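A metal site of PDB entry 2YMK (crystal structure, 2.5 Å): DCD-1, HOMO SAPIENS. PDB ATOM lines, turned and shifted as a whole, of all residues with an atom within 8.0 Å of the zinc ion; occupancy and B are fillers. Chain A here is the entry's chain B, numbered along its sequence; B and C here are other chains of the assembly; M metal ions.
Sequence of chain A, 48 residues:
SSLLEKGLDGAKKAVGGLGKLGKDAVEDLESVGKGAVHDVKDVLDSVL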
ATOM      1  N   GLY A  35      28.147   7.877  30.071  1.00  0.00           N
ATOM      2  CA  GLY A  35      29.264   7.937  29.150  1.00  0.00           C
ATOM      3  C   GLY A  35      29.509   6.576  28.572  1.00  0.00           C
ATOM      4  O   GLY A  35      29.390   6.382  27.383  1.00  0.00           O
ATOM      5  N   VAL A  37      27.611   3.934  28.441  1.00  0.00           N
ATOM      6  CA  VAL A  37      26.514   3.583  27.552  1.00  0.00           C
ATOM      7  C   VAL A  37      26.698   4.237  26.196  1.00  0.00           C
ATOM      8  O   VAL A  37      27.065   3.562  25.279  1.00  0.00           O
ATOM      9  CB  VAL A  37      25.137   3.860  28.161  1.00  0.00           C
ATOM     10  CG1 VAL A  37      24.037   3.452  27.140  1.00  0.00           C
ATOM     11  CG2 VAL A  37      25.005   3.137  29.567  1.00  0.00           C
ATOM     12  N   HIS A  38      26.497   5.533  26.039  1.00  0.00           N
ATOM     13  CA  HIS A  38      26.626   6.137  24.696  1.00  0.00           C
ATOM     14  C   HIS A  38      27.798   5.567  23.936  1.00  0.00           C
ATOM     15  O   HIS A  38      27.660   5.239  22.760  1.00  0.00           O
ATOM     16  CB  HIS A  38      26.802   7.641  24.755  1.00  0.00           C
ATOM     17  CG  HIS A  38      26.699   8.321  23.413  1.00  0.00           C
ATOM     18  ND1 HIS A  38      25.615   8.148  22.564  1.00  0.00           N
ATOM     19  CD2 HIS A  38      27.540   9.172  22.774  1.00  0.00           C
ATOM     20  CE1 HIS A  38      25.815   8.841  21.446  1.00  0.00           C
ATOM     21  NE2 HIS A  38      26.971   9.469  21.547  1.00  0.00           N
ATOM     22  N   ASP A  39      28.949   5.467  24.599  1.00  0.00           N
ATOM     23  CA  ASP A  39      30.191   4.924  24.049  1.00  0.00           C
ATOM     24  C   ASP A  39      30.069   3.469  23.558  1.00  0.00           C
ATOM     25  O   ASP A  39      30.700   3.113  22.567  1.00  0.00           O
ATOM     26  CB  ASP A  39      31.325   5.077  25.070  1.00  0.00           C
ATOM     27  CG  ASP A  39      31.986   6.486  25.071  1.00  0.00           C
ATOM     28  OD1 ASP A  39      31.903   7.228  24.043  1.00  0.00           O
ATOM     29  OD2 ASP A  39      32.656   6.812  26.086  1.00  0.00           O
ATOM     30  N   VAL A  40      29.256   2.628  24.208  1.00  0.00           N
ATOM     31  CA  VAL A  40      28.928   1.299  23.667  1.00  0.00           C
ATOM     32  C   VAL A  40      27.934   1.318  22.539  1.00  0.00           C
ATOM     33  O   VAL A  40      28.010   0.548  21.654  1.00  0.00           O
ATOM     34  CB  VAL A  40      28.300   0.382  24.677  1.00  0.00           C
ATOM     35  CG1 VAL A  40      28.157  -0.985  24.052  1.00  0.00           C
ATOM     36  CG2 VAL A  40      29.114   0.294  25.927  1.00  0.00           C
ATOM     37  N   LYS A  41      26.923   2.146  22.614  1.00  0.00           N
ATOM     38  CA  LYS A  41      26.070   2.408  21.471  1.00  0.00           C
ATOM     39  C   LYS A  41      26.856   2.754  20.221  1.00  0.00           C
ATOM     40  O   LYS A  41      26.412   2.400  19.139  1.00  0.00           O
ATOM     41  CB  LYS A  41      25.121   3.563  21.720  1.00  0.00           C
ATOM     42  CG  LYS A  41      23.900   3.228  22.487  1.00  0.00           C
ATOM     43  CD  LYS A  41      22.786   4.031  21.904  1.00  0.00           C
ATOM     44  CE  LYS A  41      22.031   4.721  22.976  1.00  0.00           C
ATOM     45  NZ  LYS A  41      21.854   6.088  22.446  1.00  0.00           N
ATOM     46  N   ASP A  42      27.983   3.480  20.357  1.00  0.00           N
ATOM     47  CA  ASP A  42      28.892   3.806  19.232  1.00  0.00           C
ATOM     48  C   ASP A  42      29.577   2.578  18.671  1.00  0.00           C
ATOM     49  O   ASP A  42      29.533   2.350  17.483  1.00  0.00           O
ATOM     50  CB  ASP A  42      29.947   4.823  19.628  1.00  0.00           C
ATOM     51  CG  ASP A  42      29.388   6.214  19.788  1.00  0.00           C
ATOM     52  OD1 ASP A  42      28.181   6.428  19.548  1.00  0.00           O
ATOM     53  OD2 ASP A  42      30.170   7.116  20.148  1.00  0.00           O
ATOM     54  N   VAL A  43      30.199   1.765  19.506  1.00  0.00           N
ATOM     55  CA  VAL A  43      30.787   0.518  19.044  1.00  0.00           C
ATOM     56  C   VAL A  43      29.800  -0.394  18.355  1.00  0.00           C
ATOM     57  O   VAL A  43      30.106  -0.908  17.307  1.00  0.00           O
ATOM     58  CB  VAL A  43      31.424  -0.262  20.191  1.00  0.00           C
ATOM     59  CG1 VAL A  43      31.766  -1.659  19.741  1.00  0.00           C
ATOM     60  CG2 VAL A  43      32.671   0.478  20.681  1.00  0.00           C
ATOM     61  N   ASP A  45      26.903   0.242  16.930  1.00  0.00           N
ATOM     62  CA  ASP A  45      26.585   1.005  15.712  1.00  0.00           C
ATOM     63  C   ASP A  45      27.686   0.843  14.638  1.00  0.00           C
ATOM     64  O   ASP A  45      27.396   0.730  13.443  1.00  0.00           O
ATOM     65  CB  ASP A  45      26.542   2.492  16.112  1.00  0.00           C
ATOM     66  CG  ASP A  45      25.335   3.278  15.548  1.00  0.00           C
ATOM     67  OD1 ASP A  45      24.934   3.066  14.380  1.00  0.00           O
ATOM     68  OD2 ASP A  45      24.828   4.168  16.288  1.00  0.00           O
ATOM     69  N   LEU B   4      35.386  11.198  13.836  1.00  0.00           N
ATOM     70  CA  LEU B   4      34.492  12.370  13.850  1.00  0.00           C
ATOM     71  C   LEU B   4      33.563  12.219  14.999  1.00  0.00           C
ATOM     72  O   LEU B   4      33.391  13.126  15.813  1.00  0.00           O
ATOM     73  CB  LEU B   4      33.620  12.382  12.597  1.00  0.00           C
ATOM     74  CG  LEU B   4      33.876  13.299  11.407  1.00  0.00           C
ATOM     75  CD1 LEU B   4      33.172  12.790  10.089  1.00  0.00           C
ATOM     76  CD2 LEU B   4      33.519  14.772  11.741  1.00  0.00           C
ATOM     77  N   GLU B   5      32.925  11.054  15.053  1.00  0.00           N
ATOM     78  CA  GLU B   5      31.968  10.773  16.081  1.00  0.00           C
ATOM     79  C   GLU B   5      32.696  11.004  17.355  1.00  0.00           C
ATOM     80  O   GLU B   5      32.229  11.726  18.230  1.00  0.00           O
ATOM     81  CB  GLU B   5      31.442   9.350  15.976  1.00  0.00           C
ATOM     82  CG  GLU B   5      29.975   9.299  15.573  1.00  0.00           C
ATOM     83  CD  GLU B   5      29.042   9.846  16.666  1.00  0.00           C
ATOM     84  OE1 GLU B   5      29.504  10.171  17.767  1.00  0.00           O
ATOM     85  OE2 GLU B   5      27.829   9.913  16.427  1.00  0.00           O
ATOM     86  N   LYS B   6      33.891  10.460  17.435  1.00  0.00           N
ATOM     87  CA  LYS B   6      34.655  10.489  18.644  1.00  0.00           C
ATOM     88  C   LYS B   6      34.911  11.952  19.023  1.00  0.00           C
ATOM     89  O   LYS B   6      35.030  12.260  20.185  1.00  0.00           O
ATOM     90  CB  LYS B   6      35.927   9.634  18.449  1.00  0.00           C
ATOM     91  CG  LYS B   6      36.385   8.767  19.666  1.00  0.00           C
ATOM     92  CD  LYS B   6      35.589   7.464  19.959  1.00  0.00           C
ATOM     93  CE  LYS B   6      35.994   6.903  21.359  1.00  0.00           C
ATOM     94  NZ  LYS B   6      36.248   5.414  21.411  1.00  0.00           N
ATOM     95  N   GLY B   7      34.919  12.857  18.066  1.00  0.00           N
ATOM     96  CA  GLY B   7      35.181  14.268  18.314  1.00  0.00           C
ATOM     97  C   GLY B   7      33.970  15.067  18.744  1.00  0.00           C
ATOM     98  O   GLY B   7      34.068  16.027  19.474  1.00  0.00           O
ATOM     99  N   LEU B   8      32.807  14.669  18.281  1.00  0.00           N
ATOM    100  CA  LEU B   8      31.567  15.257  18.735  1.00  0.00           C
ATOM    101  C   LEU B   8      31.387  14.914  20.184  1.00  0.00           C
ATOM    102  O   LEU B   8      31.021  15.769  20.969  1.00  0.00           O
ATOM    103  CB  LEU B   8      30.410  14.691  17.914  1.00  0.00           C
ATOM    104  CG  LEU B   8      30.782  14.850  16.435  1.00  0.00           C
ATOM    105  CD1 LEU B   8      30.045  13.897  15.613  1.00  0.00           C
ATOM    106  CD2 LEU B   8      30.635  16.287  15.883  1.00  0.00           C
ATOM    107  N   ASP B   9      31.661  13.663  20.536  1.00  0.00           N
ATOM    108  CA  ASP B   9      31.567  13.207  21.914  1.00  0.00           C
ATOM    109  C   ASP B   9      32.690  13.806  22.777  1.00  0.00           C
ATOM    110  O   ASP B   9      32.689  13.657  23.991  1.00  0.00           O
ATOM    111  CB  ASP B   9      31.582  11.653  22.000  1.00  0.00           C
ATOM    112  CG  ASP B   9      30.276  10.961  21.453  1.00  0.00           C
ATOM    113  OD1 ASP B   9      29.242  11.639  21.184  1.00  0.00           O
ATOM    114  OD2 ASP B   9      30.282   9.708  21.292  1.00  0.00           O
ATOM    115  N   GLY B  10      33.658  14.462  22.149  1.00  0.00           N
ATOM    116  CA  GLY B  10      34.680  15.208  22.878  1.00  0.00           C
ATOM    117  C   GLY B  10      34.124  16.562  23.249  1.00  0.00           C
ATOM    118  O   GLY B  10      34.058  16.902  24.403  1.00  0.00           O
ATOM    119  N   LYS B  12      30.900  17.461  23.203  1.00  0.00           N
ATOM    120  CA  LYS B  12      29.784  17.182  24.153  1.00  0.00           C
ATOM    121  C   LYS B  12      30.253  16.947  25.613  1.00  0.00           C
ATOM    122  O   LYS B  12      29.586  17.381  26.571  1.00  0.00           O
ATOM    123  CB  LYS B  12      28.932  15.973  23.701  1.00  0.00           C
ATOM    124  CG  LYS B  12      27.446  16.078  24.073  1.00  0.00           C
ATOM    125  CD  LYS B  12      26.730  14.761  24.502  1.00  0.00           C
ATOM    126  CE  LYS B  12      27.023  13.496  23.635  1.00  0.00           C
ATOM    127  NZ  LYS B  12      25.954  12.470  23.806  1.00  0.00           N
ATOM    128  N   LYS C  41      26.064  16.199  14.499  1.00  0.00           N
ATOM    129  CA  LYS C  41      25.929  14.788  14.301  1.00  0.00           C
ATOM    130  C   LYS C  41      24.711  14.412  13.420  1.00  0.00           C
ATOM    131  O   LYS C  41      24.768  13.443  12.698  1.00  0.00           O
ATOM    132  CB  LYS C  41      25.870  14.065  15.660  1.00  0.00           C
HETATM  133 ZN    ZN M   1      28.854   9.021  20.172  1.00  0.00          ZN
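Within 4 Å of the zinc ion: His 38, Asp 42, Glu 5 of chain B and Asp 9 of chain B.
The zinc ion is bound by the side-chain carboxylate (OD2) of Asp 9 of chain B, the side-chain carboxylate (OD2) of Asp 42 and a ring nitrogen (NE2) of His 38.
The zinc ion has three donor atoms within binding distance.
Slightly farther from the zinc ion lies the side-chain carboxylate (OE1) of Glu 5 of chain B (2.7 Å).
Slightly farther from the zinc ion lies OD1 of Asp 42 (2.8 Å).
Slightly farther from the zinc ion lies the side-chain carboxylate (OD1) of Asp 9 of chain B (2.8 Å).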
